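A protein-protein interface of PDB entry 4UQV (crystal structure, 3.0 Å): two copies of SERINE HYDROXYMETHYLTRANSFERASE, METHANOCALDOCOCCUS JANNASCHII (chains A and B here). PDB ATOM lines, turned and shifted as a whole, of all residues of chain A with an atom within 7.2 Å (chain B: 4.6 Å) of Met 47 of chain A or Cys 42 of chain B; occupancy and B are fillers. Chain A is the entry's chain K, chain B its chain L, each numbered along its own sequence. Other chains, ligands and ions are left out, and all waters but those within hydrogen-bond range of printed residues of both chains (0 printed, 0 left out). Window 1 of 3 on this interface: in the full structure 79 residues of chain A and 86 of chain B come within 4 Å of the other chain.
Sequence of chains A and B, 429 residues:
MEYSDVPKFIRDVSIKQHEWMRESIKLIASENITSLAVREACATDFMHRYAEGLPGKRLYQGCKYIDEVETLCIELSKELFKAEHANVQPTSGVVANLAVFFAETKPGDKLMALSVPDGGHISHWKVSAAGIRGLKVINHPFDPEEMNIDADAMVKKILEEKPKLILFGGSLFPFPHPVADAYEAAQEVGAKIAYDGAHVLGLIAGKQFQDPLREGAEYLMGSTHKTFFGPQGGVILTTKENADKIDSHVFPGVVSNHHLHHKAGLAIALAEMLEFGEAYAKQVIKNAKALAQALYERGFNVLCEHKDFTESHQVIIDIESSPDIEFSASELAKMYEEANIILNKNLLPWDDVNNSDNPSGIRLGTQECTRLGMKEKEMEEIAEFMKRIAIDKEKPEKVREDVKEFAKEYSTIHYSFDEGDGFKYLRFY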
ATOM      1  N   VAL A  38     -22.246   8.349  -5.967  1.00  0.00           N
ATOM      2  CA  VAL A  38     -20.987   7.915  -6.554  1.00  0.00           C
ATOM      3  C   VAL A  38     -19.909   8.994  -6.422  1.00  0.00           C
ATOM      4  O   VAL A  38     -18.727   8.684  -6.271  1.00  0.00           O
ATOM      5  CB  VAL A  38     -21.181   7.524  -8.039  1.00  0.00           C
ATOM      6  CG1 VAL A  38     -22.423   6.671  -8.184  1.00  0.00           C
ATOM      7  CG2 VAL A  38     -21.305   8.749  -8.925  1.00  0.00           C
ATOM      8  N   ARG A  39     -20.320  10.257  -6.449  1.00  0.00           N
ATOM      9  CA  ARG A  39     -19.383  11.368  -6.354  1.00  0.00           C
ATOM     10  C   ARG A  39     -18.848  11.484  -4.933  1.00  0.00           C
ATOM     11  O   ARG A  39     -17.678  11.795  -4.719  1.00  0.00           O
ATOM     12  CB  ARG A  39     -20.060  12.660  -6.799  1.00  0.00           C
ATOM     13  CG  ARG A  39     -19.629  13.908  -6.069  1.00  0.00           C
ATOM     14  CD  ARG A  39     -20.230  15.113  -6.758  1.00  0.00           C
ATOM     15  NE  ARG A  39     -21.470  14.759  -7.444  1.00  0.00           N
ATOM     16  CZ  ARG A  39     -21.997  15.460  -8.439  1.00  0.00           C
ATOM     17  NH1 ARG A  39     -21.388  16.555  -8.872  1.00  0.00           N
ATOM     18  NH2 ARG A  39     -23.129  15.065  -9.007  1.00  0.00           N
ATOM     19  N   GLU A  40     -19.717  11.223  -3.965  1.00  0.00           N
ATOM     20  CA  GLU A  40     -19.305  11.109  -2.574  1.00  0.00           C
ATOM     21  C   GLU A  40     -18.405   9.897  -2.395  1.00  0.00           C
ATOM     22  O   GLU A  40     -17.351   9.977  -1.761  1.00  0.00           O
ATOM     23  CB  GLU A  40     -20.522  10.992  -1.661  1.00  0.00           C
ATOM     24  CG  GLU A  40     -20.201  10.549  -0.251  1.00  0.00           C
ATOM     25  CD  GLU A  40     -21.414   9.996   0.461  1.00  0.00           C
ATOM     26  OE1 GLU A  40     -22.546  10.293   0.023  1.00  0.00           O
ATOM     27  OE2 GLU A  40     -21.238   9.259   1.451  1.00  0.00           O
ATOM     28  N   ALA A  41     -18.833   8.775  -2.967  1.00  0.00           N
ATOM     29  CA  ALA A  41     -18.126   7.507  -2.823  1.00  0.00           C
ATOM     30  C   ALA A  41     -16.726   7.541  -3.425  1.00  0.00           C
ATOM     31  O   ALA A  41     -15.853   6.779  -3.014  1.00  0.00           O
ATOM     32  CB  ALA A  41     -18.932   6.392  -3.453  1.00  0.00           C
ATOM     33  N   CYS A  42     -16.516   8.418  -4.402  1.00  0.00           N
ATOM     34  CA  CYS A  42     -15.210   8.532  -5.040  1.00  0.00           C
ATOM     35  C   CYS A  42     -14.197   9.220  -4.130  1.00  0.00           C
ATOM     36  O   CYS A  42     -12.988   9.087  -4.321  1.00  0.00           O
ATOM     37  CB  CYS A  42     -15.323   9.291  -6.363  1.00  0.00           C
ATOM     38  SG  CYS A  42     -15.931   8.294  -7.743  1.00  0.00           S
ATOM     39  N   ALA A  43     -14.697   9.948  -3.136  1.00  0.00           N
ATOM     40  CA  ALA A  43     -13.839  10.712  -2.236  1.00  0.00           C
ATOM     41  C   ALA A  43     -13.506   9.948  -0.955  1.00  0.00           C
ATOM     42  O   ALA A  43     -12.827  10.470  -0.077  1.00  0.00           O
ATOM     43  CB  ALA A  43     -14.493  12.043  -1.893  1.00  0.00           C
ATOM     44  N   THR A  44     -13.977   8.711  -0.852  1.00  0.00           N
ATOM     45  CA  THR A  44     -13.796   7.943   0.374  1.00  0.00           C
ATOM     46  C   THR A  44     -12.381   7.389   0.503  1.00  0.00           C
ATOM     47  O   THR A  44     -11.499   7.708  -0.297  1.00  0.00           O
ATOM     48  CB  THR A  44     -14.799   6.788   0.460  1.00  0.00           C
ATOM     49  OG1 THR A  44     -14.643   5.933  -0.678  1.00  0.00           O
ATOM     50  CG2 THR A  44     -16.216   7.334   0.483  1.00  0.00           C
ATOM     51  N   ASP A  45     -12.174   6.548   1.510  1.00  0.00           N
ATOM     52  CA  ASP A  45     -10.835   6.092   1.861  1.00  0.00           C
ATOM     53  C   ASP A  45     -10.385   4.918   0.998  1.00  0.00           C
ATOM     54  O   ASP A  45      -9.305   4.381   1.194  1.00  0.00           O
ATOM     55  CB  ASP A  45     -10.776   5.707   3.343  1.00  0.00           C
ATOM     56  CG  ASP A  45      -9.354   5.554   3.850  1.00  0.00           C
ATOM     57  OD1 ASP A  45      -8.658   6.583   3.992  1.00  0.00           O
ATOM     58  OD2 ASP A  45      -8.929   4.409   4.110  1.00  0.00           O
ATOM     59  N   PHE A  46     -11.205   4.519   0.033  1.00  0.00           N
ATOM     60  CA  PHE A  46     -10.842   3.404  -0.838  1.00  0.00           C
ATOM     61  C   PHE A  46      -9.620   3.713  -1.703  1.00  0.00           C
ATOM     62  O   PHE A  46      -9.104   2.832  -2.388  1.00  0.00           O
ATOM     63  CB  PHE A  46     -12.022   3.008  -1.722  1.00  0.00           C
ATOM     64  CG  PHE A  46     -13.133   2.335  -0.975  1.00  0.00           C
ATOM     65  CD1 PHE A  46     -12.906   1.149  -0.298  1.00  0.00           C
ATOM     66  CD2 PHE A  46     -14.404   2.881  -0.955  1.00  0.00           C
ATOM     67  CE1 PHE A  46     -13.925   0.523   0.389  1.00  0.00           C
ATOM     68  CE2 PHE A  46     -15.427   2.260  -0.270  1.00  0.00           C
ATOM     69  CZ  PHE A  46     -15.187   1.079   0.404  1.00  0.00           C
ATOM     70  N   MET A  47      -9.168   4.963  -1.678  1.00  0.00           N
ATOM     71  CA  MET A  47      -7.910   5.328  -2.316  1.00  0.00           C
ATOM     72  C   MET A  47      -6.749   4.689  -1.563  1.00  0.00           C
ATOM     73  O   MET A  47      -5.703   4.401  -2.146  1.00  0.00           O
ATOM     74  CB  MET A  47      -7.727   6.844  -2.347  1.00  0.00           C
ATOM     75  CG  MET A  47      -8.968   7.633  -2.700  1.00  0.00           C
ATOM     76  SD  MET A  47      -8.651   9.395  -2.496  1.00  0.00           S
ATOM     77  CE  MET A  47     -10.276  10.076  -2.803  1.00  0.00           C
ATOM     78  N   HIS A  48      -6.952   4.489  -0.262  1.00  0.00           N
ATOM     79  CA  HIS A  48      -5.964   3.890   0.633  1.00  0.00           C
ATOM     80  C   HIS A  48      -5.398   2.600   0.072  1.00  0.00           C
ATOM     81  O   HIS A  48      -4.250   2.547  -0.360  1.00  0.00           O
ATOM     82  CB  HIS A  48      -6.597   3.601   1.997  1.00  0.00           C
ATOM     83  CG  HIS A  48      -5.735   3.957   3.166  1.00  0.00           C
ATOM     84  ND1 HIS A  48      -5.442   5.261   3.507  1.00  0.00           N
ATOM     85  CD2 HIS A  48      -5.123   3.180   4.090  1.00  0.00           C
ATOM     86  CE1 HIS A  48      -4.674   5.270   4.582  1.00  0.00           C
ATOM     87  NE2 HIS A  48      -4.468   4.021   4.956  1.00  0.00           N
ATOM     88  N   ARG A  49      -6.232   1.570   0.055  1.00  0.00           N
ATOM     89  CA  ARG A  49      -5.779   0.228  -0.270  1.00  0.00           C
ATOM     90  C   ARG A  49      -5.764  -0.050  -1.768  1.00  0.00           C
ATOM     91  O   ARG A  49      -5.977   0.844  -2.588  1.00  0.00           O
ATOM     92  CB  ARG A  49      -6.660  -0.801   0.435  1.00  0.00           C
ATOM     93  CG  ARG A  49      -7.124  -0.386   1.825  1.00  0.00           C
ATOM     94  CD  ARG A  49      -8.048  -1.444   2.391  1.00  0.00           C
ATOM     95  NE  ARG A  49      -8.878  -0.974   3.495  1.00  0.00           N
ATOM     96  CZ  ARG A  49      -9.950  -1.624   3.945  1.00  0.00           C
ATOM     97  NH1 ARG A  49     -10.321  -2.765   3.379  1.00  0.00           N
ATOM     98  NH2 ARG A  49     -10.653  -1.134   4.956  1.00  0.00           N
ATOM     99  N   TYR A  50      -5.504  -1.307  -2.107  1.00  0.00           N
ATOM    100  CA  TYR A  50      -5.522  -1.764  -3.487  1.00  0.00           C
ATOM    101  C   TYR A  50      -6.204  -3.129  -3.552  1.00  0.00           C
ATOM    102  O   TYR A  50      -6.382  -3.779  -2.522  1.00  0.00           O
ATOM    103  CB  TYR A  50      -4.100  -1.811  -4.054  1.00  0.00           C
ATOM    104  CG  TYR A  50      -3.680  -0.507  -4.691  1.00  0.00           C
ATOM    105  CD1 TYR A  50      -4.594   0.252  -5.407  1.00  0.00           C
ATOM    106  CD2 TYR A  50      -2.380  -0.027  -4.573  1.00  0.00           C
ATOM    107  CE1 TYR A  50      -4.235   1.442  -5.995  1.00  0.00           C
ATOM    108  CE2 TYR A  50      -2.010   1.173  -5.162  1.00  0.00           C
ATOM    109  CZ  TYR A  50      -2.948   1.901  -5.872  1.00  0.00           C
ATOM    110  OH  TYR A  50      -2.615   3.093  -6.468  1.00  0.00           O
ATOM    111  N   HIS A 258      -5.842  -1.237  -8.849  1.00  0.00           N
ATOM    112  CA  HIS A 258      -6.614  -0.230  -9.569  1.00  0.00           C
ATOM    113  C   HIS A 258      -7.221   0.782  -8.606  1.00  0.00           C
ATOM    114  O   HIS A 258      -6.916   0.773  -7.417  1.00  0.00           O
ATOM    115  CB  HIS A 258      -7.706  -0.890 -10.414  1.00  0.00           C
ATOM    116  CG  HIS A 258      -8.291  -2.125  -9.801  1.00  0.00           C
ATOM    117  ND1 HIS A 258      -9.496  -2.126  -9.133  1.00  0.00           N
ATOM    118  CD2 HIS A 258      -7.837  -3.399  -9.759  1.00  0.00           C
ATOM    119  CE1 HIS A 258      -9.759  -3.348  -8.705  1.00  0.00           C
ATOM    120  NE2 HIS A 258      -8.768  -4.139  -9.071  1.00  0.00           N
ATOM    121  N   HIS A 259      -8.082   1.655  -9.120  1.00  0.00           N
ATOM    122  CA  HIS A 259      -8.662   2.702  -8.289  1.00  0.00           C
ATOM    123  C   HIS A 259      -9.999   2.220  -7.744  1.00  0.00           C
ATOM    124  O   HIS A 259     -10.983   2.134  -8.474  1.00  0.00           O
ATOM    125  CB  HIS A 259      -8.842   3.998  -9.085  1.00  0.00           C
ATOM    126  CG  HIS A 259      -7.668   4.353  -9.949  1.00  0.00           C
ATOM    127  ND1 HIS A 259      -6.419   3.794  -9.781  1.00  0.00           N
ATOM    128  CD2 HIS A 259      -7.558   5.211 -10.990  1.00  0.00           C
ATOM    129  CE1 HIS A 259      -5.591   4.290 -10.685  1.00  0.00           C
ATOM    130  NE2 HIS A 259      -6.257   5.153 -11.429  1.00  0.00           N
ATOM    131  N   LEU A 260     -10.031   1.947  -6.444  1.00  0.00           N
ATOM    132  CA  LEU A 260     -11.137   1.218  -5.832  1.00  0.00           C
ATOM    133  C   LEU A 260     -12.365   2.072  -5.546  1.00  0.00           C
ATOM    134  O   LEU A 260     -13.496   1.594  -5.659  1.00  0.00           O
ATOM    135  CB  LEU A 260     -10.653   0.555  -4.547  1.00  0.00           C
ATOM    136  CG  LEU A 260      -9.519  -0.429  -4.820  1.00  0.00           C
ATOM    137  CD1 LEU A 260      -8.991  -0.991  -3.527  1.00  0.00           C
ATOM    138  CD2 LEU A 260      -9.998  -1.539  -5.741  1.00  0.00           C
ATOM    139  N   HIS A 261     -12.138   3.324  -5.159  1.00  0.00           N
ATOM    140  CA  HIS A 261     -13.225   4.273  -4.940  1.00  0.00           C
ATOM    141  C   HIS A 261     -14.021   4.432  -6.224  1.00  0.00           C
ATOM    142  O   HIS A 261     -15.257   4.466  -6.218  1.00  0.00           O
ATOM    143  CB  HIS A 261     -12.680   5.623  -4.472  1.00  0.00           C
ATOM    144  CG  HIS A 261     -11.530   6.128  -5.289  1.00  0.00           C
ATOM    145  ND1 HIS A 261     -10.267   5.578  -5.216  1.00  0.00           N
ATOM    146  CD2 HIS A 261     -11.449   7.135  -6.190  1.00  0.00           C
ATOM    147  CE1 HIS A 261      -9.461   6.222  -6.039  1.00  0.00           C
ATOM    148  NE2 HIS A 261     -10.152   7.172  -6.642  1.00  0.00           N
ATOM    149  N   HIS A 262     -13.285   4.512  -7.328  1.00  0.00           N
ATOM    150  CA  HIS A 262     -13.868   4.571  -8.656  1.00  0.00           C
ATOM    151  C   HIS A 262     -14.704   3.339  -8.958  1.00  0.00           C
ATOM    152  O   HIS A 262     -15.727   3.438  -9.622  1.00  0.00           O
ATOM    153  CB  HIS A 262     -12.773   4.730  -9.710  1.00  0.00           C
ATOM    154  CG  HIS A 262     -12.334   6.146  -9.909  1.00  0.00           C
ATOM    155  ND1 HIS A 262     -13.096   7.220  -9.503  1.00  0.00           N
ATOM    156  CD2 HIS A 262     -11.216   6.665 -10.469  1.00  0.00           C
ATOM    157  CE1 HIS A 262     -12.465   8.342  -9.806  1.00  0.00           C
ATOM    158  NE2 HIS A 262     -11.324   8.032 -10.392  1.00  0.00           N
ATOM    159  N   PHE A 428     -14.842  19.728   2.734  1.00  0.00           N
ATOM    160  CA  PHE A 428     -14.245  18.738   3.621  1.00  0.00           C
ATOM    161  C   PHE A 428     -13.555  19.428   4.792  1.00  0.00           C
ATOM    162  O   PHE A 428     -13.288  18.810   5.823  1.00  0.00           O
ATOM    163  CB  PHE A 428     -13.258  17.852   2.858  1.00  0.00           C
ATOM    164  CG  PHE A 428     -13.886  16.631   2.246  1.00  0.00           C
ATOM    165  CD1 PHE A 428     -14.029  15.468   2.984  1.00  0.00           C
ATOM    166  CD2 PHE A 428     -14.337  16.646   0.935  1.00  0.00           C
ATOM    167  CE1 PHE A 428     -14.609  14.343   2.426  1.00  0.00           C
ATOM    168  CE2 PHE A 428     -14.915  15.522   0.370  1.00  0.00           C
ATOM    169  CZ  PHE A 428     -15.052  14.369   1.118  1.00  0.00           C
ATOM    170  N   THR B  34      -4.670  10.642   2.344  1.00  0.00           N
ATOM    171  CA  THR B  34      -4.860  11.891   1.612  1.00  0.00           C
ATOM    172  C   THR B  34      -5.556  12.943   2.472  1.00  0.00           C
ATOM    173  O   THR B  34      -6.538  12.648   3.152  1.00  0.00           O
ATOM    174  CB  THR B  34      -5.677  11.670   0.332  1.00  0.00           C
ATOM    175  OG1 THR B  34      -6.919  11.035   0.662  1.00  0.00           O
ATOM    176  CG2 THR B  34      -4.915  10.787  -0.637  1.00  0.00           C
ATOM    177  N   VAL B  38      -6.775  17.778  -0.316  1.00  0.00           N
ATOM    178  CA  VAL B  38      -6.566  16.921  -1.477  1.00  0.00           C
ATOM    179  C   VAL B  38      -7.832  16.133  -1.794  1.00  0.00           C
ATOM    180  O   VAL B  38      -8.283  16.088  -2.939  1.00  0.00           O
ATOM    181  CB  VAL B  38      -5.400  15.936  -1.254  1.00  0.00           C
ATOM    182  CG1 VAL B  38      -5.418  14.845  -2.308  1.00  0.00           C
ATOM    183  CG2 VAL B  38      -4.068  16.672  -1.261  1.00  0.00           C
ATOM    184  N   ARG B  39      -8.404  15.528  -0.759  1.00  0.00           N
ATOM    185  CA  ARG B  39      -9.566  14.659  -0.896  1.00  0.00           C
ATOM    186  C   ARG B  39     -10.812  15.409  -1.368  1.00  0.00           C
ATOM    187  O   ARG B  39     -11.746  14.808  -1.900  1.00  0.00           O
ATOM    188  CB  ARG B  39      -9.853  13.967   0.438  1.00  0.00           C
ATOM    189  CG  ARG B  39     -10.877  12.859   0.356  1.00  0.00           C
ATOM    190  CD  ARG B  39     -11.716  12.785   1.616  1.00  0.00           C
ATOM    191  NE  ARG B  39     -11.009  12.180   2.740  1.00  0.00           N
ATOM    192  CZ  ARG B  39     -11.618  11.658   3.800  1.00  0.00           C
ATOM    193  NH1 ARG B  39     -12.942  11.660   3.874  1.00  0.00           N
ATOM    194  NH2 ARG B  39     -10.906  11.127   4.783  1.00  0.00           N
ATOM    195  N   GLU B  40     -10.822  16.723  -1.174  1.00  0.00           N
ATOM    196  CA  GLU B  40     -11.994  17.535  -1.487  1.00  0.00           C
ATOM    197  C   GLU B  40     -12.203  17.701  -2.986  1.00  0.00           C
ATOM    198  O   GLU B  40     -13.337  17.722  -3.467  1.00  0.00           O
ATOM    199  CB  GLU B  40     -11.871  18.909  -0.830  1.00  0.00           C
ATOM    200  CG  GLU B  40     -13.186  19.647  -0.672  1.00  0.00           C
ATOM    201  CD  GLU B  40     -13.019  20.958   0.067  1.00  0.00           C
ATOM    202  OE1 GLU B  40     -12.488  21.915  -0.536  1.00  0.00           O
ATOM    203  OE2 GLU B  40     -13.412  21.031   1.251  1.00  0.00           O
ATOM    204  N   ALA B  41     -11.099  17.819  -3.717  1.00  0.00           N
ATOM    205  CA  ALA B  41     -11.145  18.080  -5.152  1.00  0.00           C
ATOM    206  C   ALA B  41     -11.618  16.868  -5.949  1.00  0.00           C
ATOM    207  O   ALA B  41     -12.013  16.994  -7.108  1.00  0.00           O
ATOM    208  CB  ALA B  41      -9.776  18.527  -5.643  1.00  0.00           C
ATOM    209  N   CYS B  42     -11.582  15.696  -5.323  1.00  0.00           N
ATOM    210  CA  CYS B  42     -11.915  14.452  -6.006  1.00  0.00           C
ATOM    211  C   CYS B  42     -13.395  14.360  -6.387  1.00  0.00           C
ATOM    212  O   CYS B  42     -13.756  13.650  -7.326  1.00  0.00           O
ATOM    213  CB  CYS B  42     -11.529  13.256  -5.133  1.00  0.00           C
ATOM    214  SG  CYS B  42      -9.785  13.219  -4.649  1.00  0.00           S
ATOM    215  N   ALA B  43     -14.245  15.075  -5.658  1.00  0.00           N
ATOM    216  CA  ALA B  43     -15.687  15.006  -5.883  1.00  0.00           C
ATOM    217  C   ALA B  43     -16.172  16.060  -6.876  1.00  0.00           C
ATOM    218  O   ALA B  43     -17.328  16.047  -7.291  1.00  0.00           O
ATOM    219  CB  ALA B  43     -16.427  15.148  -4.562  1.00  0.00           C
ATOM    220  N   THR B  44     -15.279  16.960  -7.270  1.00  0.00           N
ATOM    221  CA  THR B  44     -15.650  18.090  -8.114  1.00  0.00           C
ATOM    222  C   THR B  44     -16.083  17.671  -9.518  1.00  0.00           C
ATOM    223  O   THR B  44     -15.821  16.552  -9.956  1.00  0.00           O
ATOM    224  CB  THR B  44     -14.491  19.100  -8.231  1.00  0.00           C
ATOM    225  OG1 THR B  44     -13.255  18.397  -8.395  1.00  0.00           O
ATOM    226  CG2 THR B  44     -14.410  19.960  -6.983  1.00  0.00           C
ATOM    227  N   MET B  47     -14.549  15.517 -12.717  1.00  0.00           N
ATOM    228  CA  MET B  47     -14.735  14.105 -13.037  1.00  0.00           C
ATOM    229  C   MET B  47     -15.292  13.887 -14.437  1.00  0.00           C
ATOM    230  O   MET B  47     -15.055  12.848 -15.052  1.00  0.00           O
ATOM    231  CB  MET B  47     -15.674  13.444 -12.027  1.00  0.00           C
ATOM    232  CG  MET B  47     -15.093  13.281 -10.641  1.00  0.00           C
ATOM    233  SD  MET B  47     -15.799  11.876  -9.758  1.00  0.00           S
ATOM    234  CE  MET B  47     -17.420  12.508  -9.347  1.00  0.00           C
ATOM    235  N   GLN B 232      -4.823   9.515  -7.330  1.00  0.00           N
ATOM    236  CA  GLN B 232      -4.307   8.410  -8.121  1.00  0.00           C
ATOM    237  C   GLN B 232      -3.828   8.930  -9.469  1.00  0.00           C
ATOM    238  O   GLN B 232      -4.480   9.773 -10.084  1.00  0.00           O
ATOM    239  CB  GLN B 232      -5.375   7.333  -8.313  1.00  0.00           C
ATOM    240  CG  GLN B 232      -4.967   5.947  -7.839  1.00  0.00           C
ATOM    241  CD  GLN B 232      -5.129   5.758  -6.343  1.00  0.00           C
ATOM    242  OE1 GLN B 232      -5.182   6.725  -5.581  1.00  0.00           O
ATOM    243  NE2 GLN B 232      -5.220   4.504  -5.915  1.00  0.00           N
ATOM    244  N   HIS B 261     -10.318  15.512 -11.900  1.00  0.00           N
ATOM    245  CA  HIS B 261     -10.594  15.645 -10.476  1.00  0.00           C
ATOM    246  C   HIS B 261      -9.370  15.265  -9.643  1.00  0.00           C
ATOM    247  O   HIS B 261      -8.936  16.011  -8.751  1.00  0.00           O
ATOM    248  CB  HIS B 261     -11.805  14.785 -10.093  1.00  0.00           C
ATOM    249  CG  HIS B 261     -11.727  13.362 -10.564  1.00  0.00           C
ATOM    250  ND1 HIS B 261     -11.371  13.013 -11.849  1.00  0.00           N
ATOM    251  CD2 HIS B 261     -12.005  12.200  -9.925  1.00  0.00           C
ATOM    252  CE1 HIS B 261     -11.406  11.699 -11.974  1.00  0.00           C
ATOM    253  NE2 HIS B 261     -11.791  11.182 -10.823  1.00  0.00           N
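OH of Tyr 50 of chain A lies within hydrogen-bond range of NE2 of Gln 232 of chain B (3.0 Å). A ring nitrogen (NE2) of His 262 of chain A lies close to a ring nitrogen (NE2) of His 261 of chain B, at 3.2 Å. N of Phe 428 of chain A is in hydrogen-bond range of OE2 of Glu 40 of chain B (2.4 Å).
A ring nitrogen (ND1) of His 262 of chain A is in hydrogen-bond range of the side-chain sulfur of Cys 42 of chain A (3.5 Å). O of Val 38 of chain B lies within hydrogen-bond range of SG of Cys 42 of chain B (3.7 Å). The backbone carbonyl oxygen (O) of Arg 39 of chain B sits close to the side-chain sulfur (SG) of Cys 42 of chain B (3.7 Å).
Among the printed residues, pairs that only touch across the chains: Arg 39 of chain A with Ala 43 of chain B, Arg 39 of chain A with Met 47 of chain B, Ala 43 of chain A with Arg 39 of chain B, Met 47 of chain A with Thr 34 of chain B, Met 47 of chain A with Cys 42 of chain B, Met 47 of chain A with Gln 232 of chain B, His 259 of chain A with Gln 232 of chain B and Phe 428 of chain A with Arg 39 of chain B.
Asp 45 of chain A touches none of the printed residues of chain B. Of chain B, only Thr 34 (3.96 Å), Cys 42 (3.7 Å) and Gln 232 (3.8 Å) come within 4 Å of Met 47 of chain A. Arg 49 of chain A touches none of the printed residues of chain B. Printed residues of chain A within 4 Å of Thr 34 of chain B: Met 47. Cys 42 of chain B touches just one residue of chain A: Met 47. Of the printed residues of chain A, Ala 43 of chain B touches Arg 39. Of the printed residues of chain A, Met 47 of chain B touches Arg 39 (3.7 Å). Of the printed residues of chain A, His 261 of chain B touches His 262. The nearest residue of chain B that does not touch Met 47 of chain A is Arg 39 of chain B (4.3 Å). The nearest printed residue of chain A that does not touch Cys 42 of chain B is Cys 42 of chain A (4.5 Å). The nearest printed residue of chain A that does not touch Thr 34 of chain B is His 48 of chain A (5.6 Å).
Of the 19 printed residues of chain A, 7 touch a printed residue of chain B. Printed residues of chain A that touch a printed residue of chain B: Arg 39, Ala 43, Met 47, Tyr 50, His 259, His 262 and Phe 428. Among the printed residues, no Asp or Glu carboxylate lies within 4 Å of a Lys or Arg side-chain nitrogen of the other chain.
Arg 39 of chain A touches Ala 43 of chain B, and with the chains exchanged Ala 43 of chain A touches Arg 39 of chain B. Arg 39 of chain A touches Met 47 of chain B, but with the chains exchanged Met 47 of chain A does not touch Arg 39 of chain B (4.3 Å). Met 47 of chain A touches Cys 42 of chain B, but with the chains exchanged Cys 42 of chain A does not touch Met 47 of chain B (4.1 Å).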
